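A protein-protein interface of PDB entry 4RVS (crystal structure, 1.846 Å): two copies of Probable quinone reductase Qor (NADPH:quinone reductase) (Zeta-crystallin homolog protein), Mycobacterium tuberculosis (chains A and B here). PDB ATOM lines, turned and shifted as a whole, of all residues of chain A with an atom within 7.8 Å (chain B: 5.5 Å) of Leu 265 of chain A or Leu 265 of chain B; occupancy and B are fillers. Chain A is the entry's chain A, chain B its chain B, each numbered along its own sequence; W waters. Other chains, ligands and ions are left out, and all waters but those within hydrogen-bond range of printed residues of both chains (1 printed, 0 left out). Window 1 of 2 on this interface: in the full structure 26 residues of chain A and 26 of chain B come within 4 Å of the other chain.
The backbone carbonyl oxygen (O) of Val 137 of chain A is in hydrogen-bond range of the side-chain hydroxyl (OH) of Tyr 264 of chain B (2.7 Å).
O of Val 252 of chain A sits at hydrogen-bond distance from N of Val 252 of chain B (2.8 Å).
NH2 of Arg 267 of chain B sits close to NE2 of Gln 255 of chain A, 3.4 Å away.
The backbone carbonyl oxygen of Val 263 of chain A sits at hydrogen-bond distance from the side-chain hydroxyl of Thr 266 of chain B (2.9 Å).
The backbone NH (N) of Leu 265 of chain A sits at hydrogen-bond distance from the backbone carbonyl oxygen (O) of Leu 265 of chain B, 2.7 Å away.
The side-chain hydroxyl (OG1) of Thr 266 of chain A is in hydrogen-bond range of the backbone carbonyl oxygen (O) of Val 263 of chain B (2.8 Å).
O of Gly 237 of chain A lies within hydrogen-bond range of N of Tyr 264 of chain A, at 2.9 Å.
The backbone carbonyl oxygen of Tyr 264 of chain A lies within hydrogen-bond range of the backbone NH of Leu 239 of chain A, at 2.8 Å.
N of Thr 266 of chain A lies within hydrogen-bond range of O of Leu 239 of chain A, at 3.0 Å.
O of Tyr 264 of chain B sits at hydrogen-bond distance from N of Leu 239 of chain B.
The backbone carbonyl oxygen of Thr 266 of chain B lies within hydrogen-bond range of the backbone NH of Leu 241 of chain B (3.0 Å).
N of Val 263 of chain B sits at hydrogen-bond distance from O of Leu 257 of chain B (3.1 Å).
Among the printed residues, merely in contact across the chains: Leu 241 of chain A with Pro 254 of chain B, Val 249 of chain A with Pro 254 of chain B, Pro 251 of chain A with Val 252 of chain B, Val 252 of chain A with Pro 254 of chain B, Pro 254 of chain A with Leu 241 of chain B, Pro 254 of chain A with Val 252 of chain B, Pro 254 of chain A with Arg 267 of chain B, Leu 257 of chain A with Leu 265 of chain B, Ser 262 of chain A with Thr 266 of chain B, Ser 262 of chain A with Arg 267 of chain B, Val 263 of chain A with Leu 265 of chain B, Tyr 264 of chain A with Leu 265 of chain B, Tyr 264 of chain A with Thr 266 of chain B, Leu 265 of chain A with Leu 257 of chain B, Leu 265 of chain A with Val 263 of chain B, Leu 265 of chain A with Tyr 264 of chain B, Thr 266 of chain A with Tyr 264 of chain B and Arg 267 of chain A with Pro 254 of chain B.
Ala 240 of chain A touches none of the printed residues of chain B.
Of the printed residues of chain B, Pro 251 of chain A touches Val 252 (3.4 Å).
Leu 265 of chain A touches just these residues of chain B: Leu 257 (3.6 Å), Val 263 (3.98 Å), Tyr 264 (3.5 Å) and Leu 265 (2.7 Å).
Printed residues of chain B within 4 Å of Arg 267 of chain A: Pro 254 (3.4 Å).
Phe 226 of chain B touches none of the printed residues of chain A.
Printed residues of chain A within 4 Å of Leu 265 of chain B: Leu 257 (3.8 Å), Val 263 (3.99 Å), Tyr 264 (3.5 Å) and Leu 265 (2.7 Å).
Printed residues of chain A within 4 Å of Arg 267 of chain B: Pro 254, Gln 255 and Ser 262.
The nearest printed residue of chain A that does not touch Leu 265 of chain B is Pro 254 of chain A (4.8 Å).
Of the 25 printed residues of chain A, 14 touch a printed residue of chain B.
Printed residues of chain A that touch a printed residue of chain B: Val 137, Leu 241, Val 249, Pro 251, Val 252, Pro 254, Gln 255, Leu 257, Ser 262, Val 263, Tyr 264, Leu 265, Thr 266 and Arg 267.
Hydrophobic or aromatic side chains of chain B that line the printed part of chain A: Leu 241, Val 252, Pro 254, Leu 257, Tyr 264 and Leu 265.
Along chain B the printed residues that touch a printed residue of chain A span positions 241 to 267.
Among the printed residues, 24 pairs touch across the chains.
Val 252 of chain A touches Pro 254 of chain B, and with the chains exchanged Pro 254 of chain A touches Val 252 of chain B.
Pro 254 of chain A touches Arg 267 of chain B, and with the chains exchanged Arg 267 of chain A touches Pro 254 of chain B.
Val 263 of chain A touches Thr 266 of chain B, and with the chains exchanged Thr 266 of chain A touches Val 263 of chain B.
Positions printed for both chains: 226, 239, 241, 252, 254, 257, 263, 264, 265, 266 and 267.
Of the 24 pairs that touch across the chains among the printed residues, 18 have their exchanged pair printed and touching as well.
Water W1 bridges O of Ser 262 of chain A (2.8 Å) and OG1 of Thr 266 of chain B (2.9 Å).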
ATOM      1  N   VAL A 137       4.615  39.714   1.451  1.00  0.00           N
ATOM      2  CA  VAL A 137       4.907  38.491   0.703  1.00  0.00           C
ATOM      3  C   VAL A 137       6.139  38.662  -0.186  1.00  0.00           C
ATOM      4  O   VAL A 137       7.095  37.876  -0.113  1.00  0.00           O
ATOM      5  CB  VAL A 137       3.689  38.028  -0.128  1.00  0.00           C
ATOM      6  CG1 VAL A 137       4.088  36.943  -1.120  1.00  0.00           C
ATOM      7  CG2 VAL A 137       2.576  37.517   0.789  1.00  0.00           C
ATOM      8  N   PHE A 226      -0.509  29.698 -14.215  1.00  0.00           N
ATOM      9  CA  PHE A 226       0.579  29.337 -13.298  1.00  0.00           C
ATOM     10  C   PHE A 226       1.880  28.955 -14.006  1.00  0.00           C
ATOM     11  O   PHE A 226       2.949  29.404 -13.594  1.00  0.00           O
ATOM     12  CB  PHE A 226       0.161  28.226 -12.310  1.00  0.00           C
ATOM     13  CG  PHE A 226       1.249  27.848 -11.322  1.00  0.00           C
ATOM     14  CD1 PHE A 226       1.395  28.544 -10.125  1.00  0.00           C
ATOM     15  CD2 PHE A 226       2.124  26.808 -11.596  1.00  0.00           C
ATOM     16  CE1 PHE A 226       2.403  28.198  -9.215  1.00  0.00           C
ATOM     17  CE2 PHE A 226       3.138  26.463 -10.706  1.00  0.00           C
ATOM     18  CZ  PHE A 226       3.271  27.161  -9.507  1.00  0.00           C
ATOM     19  N   LEU A 230       5.441  30.958 -13.503  1.00  0.00           N
ATOM     20  CA  LEU A 230       6.680  30.366 -13.005  1.00  0.00           C
ATOM     21  C   LEU A 230       7.816  30.589 -13.993  1.00  0.00           C
ATOM     22  O   LEU A 230       8.935  30.896 -13.605  1.00  0.00           O
ATOM     23  CB  LEU A 230       6.483  28.868 -12.743  1.00  0.00           C
ATOM     24  CG  LEU A 230       7.669  28.100 -12.160  1.00  0.00           C
ATOM     25  CD1 LEU A 230       8.120  28.730 -10.865  1.00  0.00           C
ATOM     26  CD2 LEU A 230       7.297  26.647 -11.928  1.00  0.00           C
ATOM     27  N   LEU A 233       9.861  34.384 -14.162  1.00  0.00           N
ATOM     28  CA  LEU A 233      10.505  34.968 -12.988  1.00  0.00           C
ATOM     29  C   LEU A 233      12.002  35.228 -13.147  1.00  0.00           C
ATOM     30  O   LEU A 233      12.724  34.444 -13.766  1.00  0.00           O
ATOM     31  CB  LEU A 233      10.285  34.060 -11.775  1.00  0.00           C
ATOM     32  CG  LEU A 233       8.899  34.153 -11.150  1.00  0.00           C
ATOM     33  CD1 LEU A 233       8.654  32.930 -10.278  1.00  0.00           C
ATOM     34  CD2 LEU A 233       8.781  35.430 -10.321  1.00  0.00           C
ATOM     35  N   GLY A 237      13.288  35.066  -7.817  1.00  0.00           N
ATOM     36  CA  GLY A 237      12.040  35.818  -7.755  1.00  0.00           C
ATOM     37  C   GLY A 237      10.970  35.106  -6.941  1.00  0.00           C
ATOM     38  O   GLY A 237      11.168  33.963  -6.518  1.00  0.00           O
ATOM     39  N   THR A 238       9.837  35.772  -6.711  1.00  0.00           N
ATOM     40  CA  THR A 238       8.777  35.189  -5.884  1.00  0.00           C
ATOM     41  C   THR A 238       7.481  35.064  -6.664  1.00  0.00           C
ATOM     42  O   THR A 238       7.013  36.039  -7.269  1.00  0.00           O
ATOM     43  CB  THR A 238       8.504  36.036  -4.632  1.00  0.00           C
ATOM     44  OG1 THR A 238       9.664  36.027  -3.788  1.00  0.00           O
ATOM     45  CG2 THR A 238       7.310  35.472  -3.842  1.00  0.00           C
ATOM     46  N   LEU A 239       6.920  33.861  -6.660  1.00  0.00           N
ATOM     47  CA  LEU A 239       5.616  33.609  -7.258  1.00  0.00           C
ATOM     48  C   LEU A 239       4.603  33.600  -6.123  1.00  0.00           C
ATOM     49  O   LEU A 239       4.546  32.656  -5.331  1.00  0.00           O
ATOM     50  CB  LEU A 239       5.603  32.267  -7.996  1.00  0.00           C
ATOM     51  CG  LEU A 239       4.630  32.145  -9.169  1.00  0.00           C
ATOM     52  CD1 LEU A 239       4.784  30.794  -9.854  1.00  0.00           C
ATOM     53  CD2 LEU A 239       3.172  32.351  -8.729  1.00  0.00           C
ATOM     54  N   ALA A 240       3.807  34.662  -6.042  1.00  0.00           N
ATOM     55  CA  ALA A 240       2.751  34.746  -5.037  1.00  0.00           C
ATOM     56  C   ALA A 240       1.428  34.298  -5.654  1.00  0.00           C
ATOM     57  O   ALA A 240       0.768  35.059  -6.361  1.00  0.00           O
ATOM     58  CB  ALA A 240       2.646  36.164  -4.489  1.00  0.00           C
ATOM     59  N   LEU A 241       1.061  33.046  -5.403  1.00  0.00           N
ATOM     60  CA  LEU A 241      -0.194  32.491  -5.905  1.00  0.00           C
ATOM     61  C   LEU A 241      -1.258  32.727  -4.846  1.00  0.00           C
ATOM     62  O   LEU A 241      -1.316  32.012  -3.849  1.00  0.00           O
ATOM     63  CB  LEU A 241      -0.032  30.992  -6.175  1.00  0.00           C
ATOM     64  CG  LEU A 241      -1.276  30.196  -6.591  1.00  0.00           C
ATOM     65  CD1 LEU A 241      -1.864  30.699  -7.911  1.00  0.00           C
ATOM     66  CD2 LEU A 241      -0.922  28.716  -6.704  1.00  0.00           C
ATOM     67  N   PHE A 242      -2.098  33.738  -5.044  1.00  0.00           N
ATOM     68  CA  PHE A 242      -3.013  34.142  -3.971  1.00  0.00           C
ATOM     69  C   PHE A 242      -4.480  33.916  -4.325  1.00  0.00           C
ATOM     70  O   PHE A 242      -5.378  34.273  -3.559  1.00  0.00           O
ATOM     71  CB  PHE A 242      -2.760  35.601  -3.567  1.00  0.00           C
ATOM     72  CG  PHE A 242      -3.164  36.597  -4.609  1.00  0.00           C
ATOM     73  CD1 PHE A 242      -4.404  37.224  -4.546  1.00  0.00           C
ATOM     74  CD2 PHE A 242      -2.309  36.905  -5.654  1.00  0.00           C
ATOM     75  CE1 PHE A 242      -4.782  38.143  -5.512  1.00  0.00           C
ATOM     76  CE2 PHE A 242      -2.674  37.826  -6.620  1.00  0.00           C
ATOM     77  CZ  PHE A 242      -3.909  38.444  -6.553  1.00  0.00           C
ATOM     78  N   VAL A 249      -4.382  25.054  -9.166  1.00  0.00           N
ATOM     79  CA  VAL A 249      -3.097  24.725  -9.766  1.00  0.00           C
ATOM     80  C   VAL A 249      -2.725  23.290  -9.403  1.00  0.00           C
ATOM     81  O   VAL A 249      -2.747  22.925  -8.224  1.00  0.00           O
ATOM     82  CB  VAL A 249      -2.000  25.683  -9.271  1.00  0.00           C
ATOM     83  CG1 VAL A 249      -0.613  25.250  -9.766  1.00  0.00           C
ATOM     84  CG2 VAL A 249      -2.305  27.091  -9.731  1.00  0.00           C
ATOM     85  N   PRO A 250      -2.406  22.467 -10.413  1.00  0.00           N
ATOM     86  CA  PRO A 250      -1.979  21.076 -10.190  1.00  0.00           C
ATOM     87  C   PRO A 250      -0.697  21.026  -9.367  1.00  0.00           C
ATOM     88  O   PRO A 250       0.101  21.975  -9.437  1.00  0.00           O
ATOM     89  CB  PRO A 250      -1.697  20.570 -11.609  1.00  0.00           C
ATOM     90  CG  PRO A 250      -2.563  21.417 -12.491  1.00  0.00           C
ATOM     91  CD  PRO A 250      -2.525  22.783 -11.848  1.00  0.00           C
ATOM     92  N   PRO A 251      -0.503  19.949  -8.582  1.00  0.00           N
ATOM     93  CA  PRO A 251       0.693  19.804  -7.744  1.00  0.00           C
ATOM     94  C   PRO A 251       1.967  20.109  -8.521  1.00  0.00           C
ATOM     95  O   PRO A 251       2.105  19.707  -9.676  1.00  0.00           O
ATOM     96  CB  PRO A 251       0.643  18.330  -7.333  1.00  0.00           C
ATOM     97  CG  PRO A 251      -0.823  18.033  -7.268  1.00  0.00           C
ATOM     98  CD  PRO A 251      -1.422  18.807  -8.424  1.00  0.00           C
ATOM     99  N   VAL A 252       2.878  20.832  -7.875  1.00  0.00           N
ATOM    100  CA  VAL A 252       4.048  21.391  -8.523  1.00  0.00           C
ATOM    101  C   VAL A 252       5.286  20.617  -8.109  1.00  0.00           C
ATOM    102  O   VAL A 252       5.616  20.551  -6.922  1.00  0.00           O
ATOM    103  CB  VAL A 252       4.216  22.868  -8.127  1.00  0.00           C
ATOM    104  CG1 VAL A 252       5.474  23.464  -8.761  1.00  0.00           C
ATOM    105  CG2 VAL A 252       2.979  23.660  -8.533  1.00  0.00           C
ATOM    106  N   ASP A 253       5.946  20.002  -9.085  1.00  0.00           N
ATOM    107  CA  ASP A 253       7.251  19.366  -8.879  1.00  0.00           C
ATOM    108  C   ASP A 253       8.249  20.412  -8.376  1.00  0.00           C
ATOM    109  O   ASP A 253       8.530  21.374  -9.079  1.00  0.00           O
ATOM    110  CB  ASP A 253       7.710  18.768 -10.217  1.00  0.00           C
ATOM    111  CG  ASP A 253       9.170  18.302 -10.213  1.00  0.00           C
ATOM    112  OD1 ASP A 253       9.757  18.062  -9.135  1.00  0.00           O
ATOM    113  OD2 ASP A 253       9.726  18.163 -11.324  1.00  0.00           O
ATOM    114  N   PRO A 254       8.776  20.241  -7.148  1.00  0.00           N
ATOM    115  CA  PRO A 254       9.712  21.241  -6.607  1.00  0.00           C
ATOM    116  C   PRO A 254      10.937  21.501  -7.493  1.00  0.00           C
ATOM    117  O   PRO A 254      11.465  22.619  -7.479  1.00  0.00           O
ATOM    118  CB  PRO A 254      10.141  20.629  -5.266  1.00  0.00           C
ATOM    119  CG  PRO A 254       8.962  19.802  -4.863  1.00  0.00           C
ATOM    120  CD  PRO A 254       8.434  19.212  -6.148  1.00  0.00           C
ATOM    121  N   GLN A 255      11.379  20.515  -8.270  1.00  0.00           N
ATOM    122  CA  GLN A 255      12.491  20.776  -9.184  1.00  0.00           C
ATOM    123  C   GLN A 255      12.165  21.875 -10.196  1.00  0.00           C
ATOM    124  O   GLN A 255      13.078  22.517 -10.714  1.00  0.00           O
ATOM    125  CB  GLN A 255      12.968  19.512  -9.905  1.00  0.00           C
ATOM    126  CG  GLN A 255      13.843  18.587  -9.048  1.00  0.00           C
ATOM    127  CD  GLN A 255      15.210  19.183  -8.704  1.00  0.00           C
ATOM    128  OE1 GLN A 255      15.574  20.269  -9.164  1.00  0.00           O
ATOM    129  NE2 GLN A 255      15.973  18.463  -7.892  1.00  0.00           N
ATOM    130  N   LEU A 257      10.867  24.626  -9.456  1.00  0.00           N
ATOM    131  CA  LEU A 257      11.257  25.869  -8.794  1.00  0.00           C
ATOM    132  C   LEU A 257      12.749  26.111  -8.930  1.00  0.00           C
ATOM    133  O   LEU A 257      13.200  27.262  -9.000  1.00  0.00           O
ATOM    134  CB  LEU A 257      10.855  25.851  -7.314  1.00  0.00           C
ATOM    135  CG  LEU A 257       9.385  25.561  -7.028  1.00  0.00           C
ATOM    136  CD1 LEU A 257       9.115  25.640  -5.536  1.00  0.00           C
ATOM    137  CD2 LEU A 257       8.523  26.559  -7.771  1.00  0.00           C
ATOM    138  N   SER A 262      15.845  29.031  -8.939  1.00  0.00           N
ATOM    139  CA  SER A 262      15.828  28.991  -7.477  1.00  0.00           C
ATOM    140  C   SER A 262      14.796  29.982  -6.939  1.00  0.00           C
ATOM    141  O   SER A 262      15.096  30.810  -6.082  1.00  0.00           O
ATOM    142  CB  SER A 262      17.219  29.271  -6.897  1.00  0.00           C
ATOM    143  OG  SER A 262      18.110  28.220  -7.248  1.00  0.00           O
ATOM    144  N   VAL A 263      13.580  29.895  -7.460  1.00  0.00           N
ATOM    145  CA  VAL A 263      12.550  30.863  -7.111  1.00  0.00           C
ATOM    146  C   VAL A 263      11.817  30.448  -5.852  1.00  0.00           C
ATOM    147  O   VAL A 263      12.009  29.344  -5.338  1.00  0.00           O
ATOM    148  CB  VAL A 263      11.536  31.040  -8.258  1.00  0.00           C
ATOM    149  CG1 VAL A 263      12.270  31.354  -9.552  1.00  0.00           C
ATOM    150  CG2 VAL A 263      10.687  29.786  -8.431  1.00  0.00           C
ATOM    151  N   TYR A 264      10.973  31.345  -5.362  1.00  0.00           N
ATOM    152  CA  TYR A 264      10.133  31.056  -4.212  1.00  0.00           C
ATOM    153  C   TYR A 264       8.720  30.891  -4.706  1.00  0.00           C
ATOM    154  O   TYR A 264       8.265  31.671  -5.548  1.00  0.00           O
ATOM    155  CB  TYR A 264      10.106  32.244  -3.257  1.00  0.00           C
ATOM    156  CG  TYR A 264      11.400  32.588  -2.559  1.00  0.00           C
ATOM    157  CD1 TYR A 264      11.693  32.078  -1.299  1.00  0.00           C
ATOM    158  CD2 TYR A 264      12.302  33.476  -3.134  1.00  0.00           C
ATOM    159  CE1 TYR A 264      12.871  32.430  -0.637  1.00  0.00           C
ATOM    160  CE2 TYR A 264      13.467  33.833  -2.491  1.00  0.00           C
ATOM    161  CZ  TYR A 264      13.752  33.310  -1.249  1.00  0.00           C
ATOM    162  OH  TYR A 264      14.932  33.687  -0.633  1.00  0.00           O
ATOM    163  N   LEU A 265       8.017  29.904  -4.159  1.00  0.00           N
ATOM    164  CA  LEU A 265       6.583  29.766  -4.384  1.00  0.00           C
ATOM    165  C   LEU A 265       5.887  29.908  -3.040  1.00  0.00           C
ATOM    166  O   LEU A 265       6.276  29.276  -2.051  1.00  0.00           O
ATOM    167  CB  LEU A 265       6.260  28.402  -4.994  1.00  0.00           C
ATOM    168  CG  LEU A 265       4.790  27.992  -5.045  1.00  0.00           C
ATOM    169  CD1 LEU A 265       4.010  29.003  -5.863  1.00  0.00           C
ATOM    170  CD2 LEU A 265       4.657  26.589  -5.622  1.00  0.00           C
ATOM    171  N   THR A 266       4.847  30.732  -3.000  1.00  0.00           N
ATOM    172  CA  THR A 266       4.066  30.875  -1.783  1.00  0.00           C
ATOM    173  C   THR A 266       2.580  30.952  -2.143  1.00  0.00           C
ATOM    174  O   THR A 266       2.222  31.443  -3.210  1.00  0.00           O
ATOM    175  CB  THR A 266       4.530  32.112  -0.992  1.00  0.00           C
ATOM    176  OG1 THR A 266       3.786  32.210   0.229  1.00  0.00           O
ATOM    177  CG2 THR A 266       4.334  33.379  -1.816  1.00  0.00           C
ATOM    178  N   ARG A 267       1.720  30.425  -1.283  1.00  0.00           N
ATOM    179  CA  ARG A 267       0.283  30.519  -1.512  1.00  0.00           C
ATOM    180  C   ARG A 267      -0.330  31.177  -0.292  1.00  0.00           C
ATOM    181  O   ARG A 267      -0.803  30.489   0.610  1.00  0.00           O
ATOM    182  CB  ARG A 267      -0.330  29.131  -1.721  1.00  0.00           C
ATOM    183  CG  ARG A 267      -1.650  29.105  -2.529  1.00  0.00           C
ATOM    184  CD  ARG A 267      -2.738  30.016  -1.961  1.00  0.00           C
ATOM    185  NE  ARG A 267      -3.997  29.919  -2.700  1.00  0.00           N
ATOM    186  CZ  ARG A 267      -5.070  30.660  -2.435  1.00  0.00           C
ATOM    187  NH1 ARG A 267      -5.029  31.563  -1.466  1.00  0.00           N
ATOM    188  NH2 ARG A 267      -6.181  30.503  -3.142  1.00  0.00           N
ATOM    189  N   PRO A 268      -0.329  32.513  -0.256  1.00  0.00           N
ATOM    190  CA  PRO A 268      -0.801  33.191   0.951  1.00  0.00           C
ATOM    191  C   PRO A 268      -2.307  33.362   0.970  1.00  0.00           C
ATOM    192  O   PRO A 268      -2.975  33.280  -0.072  1.00  0.00           O
ATOM    193  CB  PRO A 268      -0.157  34.573   0.839  1.00  0.00           C
ATOM    194  CG  PRO A 268      -0.141  34.834  -0.664  1.00  0.00           C
ATOM    195  CD  PRO A 268       0.213  33.462  -1.251  1.00  0.00           C
ATOM    196  N   PHE B 226      10.088  15.642   3.723  1.00  0.00           N
ATOM    197  CA  PHE B 226       9.433  16.854   3.217  1.00  0.00           C
ATOM    198  C   PHE B 226       8.088  17.148   3.881  1.00  0.00           C
ATOM    199  O   PHE B 226       7.834  18.292   4.250  1.00  0.00           O
ATOM    200  CB  PHE B 226       9.280  16.833   1.682  1.00  0.00           C
ATOM    201  CG  PHE B 226       8.629  18.082   1.118  1.00  0.00           C
ATOM    202  CD1 PHE B 226       9.393  19.205   0.822  1.00  0.00           C
ATOM    203  CD2 PHE B 226       7.260  18.130   0.895  1.00  0.00           C
ATOM    204  CE1 PHE B 226       8.796  20.357   0.306  1.00  0.00           C
ATOM    205  CE2 PHE B 226       6.650  19.278   0.394  1.00  0.00           C
ATOM    206  CZ  PHE B 226       7.425  20.394   0.094  1.00  0.00           C
ATOM    207  N   LEU B 239      10.546  27.026   3.674  1.00  0.00           N
ATOM    208  CA  LEU B 239      11.036  25.670   3.497  1.00  0.00           C
ATOM    209  C   LEU B 239      12.067  25.703   2.380  1.00  0.00           C
ATOM    210  O   LEU B 239      11.727  25.841   1.201  1.00  0.00           O
ATOM    211  CB  LEU B 239       9.891  24.719   3.138  1.00  0.00           C
ATOM    212  CG  LEU B 239      10.084  23.256   3.554  1.00  0.00           C
ATOM    213  CD1 LEU B 239       8.847  22.447   3.212  1.00  0.00           C
ATOM    214  CD2 LEU B 239      11.312  22.626   2.902  1.00  0.00           C
ATOM    215  N   LEU B 241      14.239  23.569   0.357  1.00  0.00           N
ATOM    216  CA  LEU B 241      14.526  22.200  -0.071  1.00  0.00           C
ATOM    217  C   LEU B 241      15.731  22.253  -0.995  1.00  0.00           C
ATOM    218  O   LEU B 241      15.606  22.631  -2.155  1.00  0.00           O
ATOM    219  CB  LEU B 241      13.315  21.616  -0.804  1.00  0.00           C
ATOM    220  CG  LEU B 241      13.435  20.230  -1.447  1.00  0.00           C
ATOM    221  CD1 LEU B 241      13.723  19.141  -0.408  1.00  0.00           C
ATOM    222  CD2 LEU B 241      12.150  19.903  -2.203  1.00  0.00           C
ATOM    223  N   VAL B 252       3.941  19.053  -5.265  1.00  0.00           N
ATOM    224  CA  VAL B 252       3.326  19.617  -4.079  1.00  0.00           C
ATOM    225  C   VAL B 252       2.117  20.455  -4.455  1.00  0.00           C
ATOM    226  O   VAL B 252       2.232  21.420  -5.218  1.00  0.00           O
ATOM    227  CB  VAL B 252       4.339  20.492  -3.322  1.00  0.00           C
ATOM    228  CG1 VAL B 252       3.703  21.101  -2.076  1.00  0.00           C
ATOM    229  CG2 VAL B 252       5.569  19.666  -2.963  1.00  0.00           C
ATOM    230  N   PRO B 254      -0.107  23.315  -4.210  1.00  0.00           N
ATOM    231  CA  PRO B 254       0.155  24.643  -3.633  1.00  0.00           C
ATOM    232  C   PRO B 254      -0.757  24.998  -2.454  1.00  0.00           C
ATOM    233  O   PRO B 254      -0.336  25.745  -1.562  1.00  0.00           O
ATOM    234  CB  PRO B 254      -0.097  25.594  -4.811  1.00  0.00           C
ATOM    235  CG  PRO B 254       0.236  24.767  -6.012  1.00  0.00           C
ATOM    236  CD  PRO B 254      -0.238  23.368  -5.681  1.00  0.00           C
ATOM    237  N   LEU B 257       0.752  24.757   0.912  1.00  0.00           N
ATOM    238  CA  LEU B 257       1.563  25.878   1.390  1.00  0.00           C
ATOM    239  C   LEU B 257       0.710  26.884   2.142  1.00  0.00           C
ATOM    240  O   LEU B 257       1.179  27.533   3.091  1.00  0.00           O
ATOM    241  CB  LEU B 257       2.287  26.568   0.228  1.00  0.00           C
ATOM    242  CG  LEU B 257       3.171  25.678  -0.645  1.00  0.00           C
ATOM    243  CD1 LEU B 257       3.933  26.534  -1.651  1.00  0.00           C
ATOM    244  CD2 LEU B 257       4.133  24.903   0.227  1.00  0.00           C
ATOM    245  N   VAL B 263       3.230  29.693   3.837  1.00  0.00           N
ATOM    246  CA  VAL B 263       4.679  29.543   3.895  1.00  0.00           C
ATOM    247  C   VAL B 263       5.296  29.717   2.521  1.00  0.00           C
ATOM    248  O   VAL B 263       4.593  29.810   1.515  1.00  0.00           O
ATOM    249  CB  VAL B 263       5.079  28.164   4.467  1.00  0.00           C
ATOM    250  CG1 VAL B 263       4.418  27.945   5.824  1.00  0.00           C
ATOM    251  CG2 VAL B 263       4.691  27.043   3.503  1.00  0.00           C
ATOM    252  N   TYR B 264       6.620  29.766   2.488  1.00  0.00           N
ATOM    253  CA  TYR B 264       7.344  29.840   1.230  1.00  0.00           C
ATOM    254  C   TYR B 264       8.000  28.503   0.996  1.00  0.00           C
ATOM    255  O   TYR B 264       8.571  27.925   1.925  1.00  0.00           O
ATOM    256  CB  TYR B 264       8.480  30.853   1.329  1.00  0.00           C
ATOM    257  CG  TYR B 264       8.094  32.302   1.503  1.00  0.00           C
ATOM    258  CD1 TYR B 264       7.972  33.147   0.407  1.00  0.00           C
ATOM    259  CD2 TYR B 264       7.919  32.843   2.772  1.00  0.00           C
ATOM    260  CE1 TYR B 264       7.654  34.494   0.570  1.00  0.00           C
ATOM    261  CE2 TYR B 264       7.606  34.177   2.947  1.00  0.00           C
ATOM    262  CZ  TYR B 264       7.476  34.998   1.851  1.00  0.00           C
ATOM    263  OH  TYR B 264       7.163  36.332   2.055  1.00  0.00           O
ATOM    264  N   LEU B 265       7.951  28.028  -0.245  1.00  0.00           N
ATOM    265  CA  LEU B 265       8.731  26.867  -0.656  1.00  0.00           C
ATOM    266  C   LEU B 265       9.724  27.326  -1.709  1.00  0.00           C
ATOM    267  O   LEU B 265       9.368  28.050  -2.647  1.00  0.00           O
ATOM    268  CB  LEU B 265       7.819  25.781  -1.231  1.00  0.00           C
ATOM    269  CG  LEU B 265       8.482  24.603  -1.942  1.00  0.00           C
ATOM    270  CD1 LEU B 265       9.379  23.866  -0.976  1.00  0.00           C
ATOM    271  CD2 LEU B 265       7.415  23.676  -2.505  1.00  0.00           C
ATOM    272  N   THR B 266      10.975  26.913  -1.559  1.00  0.00           N
ATOM    273  CA  THR B 266      11.990  27.235  -2.548  1.00  0.00           C
ATOM    274  C   THR B 266      12.900  26.019  -2.734  1.00  0.00           C
ATOM    275  O   THR B 266      13.111  25.249  -1.796  1.00  0.00           O
ATOM    276  CB  THR B 266      12.783  28.494  -2.125  1.00  0.00           C
ATOM    277  OG1 THR B 266      13.752  28.817  -3.130  1.00  0.00           O
ATOM    278  CG2 THR B 266      13.481  28.271  -0.786  1.00  0.00           C
ATOM    279  N   ARG B 267      13.387  25.802  -3.948  1.00  0.00           N
ATOM    280  CA  ARG B 267      14.308  24.702  -4.199  1.00  0.00           C
ATOM    281  C   ARG B 267      15.563  25.285  -4.816  1.00  0.00           C
ATOM    282  O   ARG B 267      15.701  25.302  -6.036  1.00  0.00           O
ATOM    283  CB  ARG B 267      13.688  23.672  -5.150  1.00  0.00           C
ATOM    284  CG  ARG B 267      14.261  22.238  -5.034  1.00  0.00           C
ATOM    285  CD  ARG B 267      15.770  22.162  -5.260  1.00  0.00           C
ATOM    286  NE  ARG B 267      16.295  20.797  -5.206  1.00  0.00           N
ATOM    287  CZ  ARG B 267      17.591  20.499  -5.258  1.00  0.00           C
ATOM    288  NH1 ARG B 267      18.492  21.468  -5.341  1.00  0.00           N
ATOM    289  NH2 ARG B 267      17.988  19.236  -5.216  1.00  0.00           N
HETATM  290  O   HOH W   1      16.018  30.632  -3.425  1.00  0.00           O
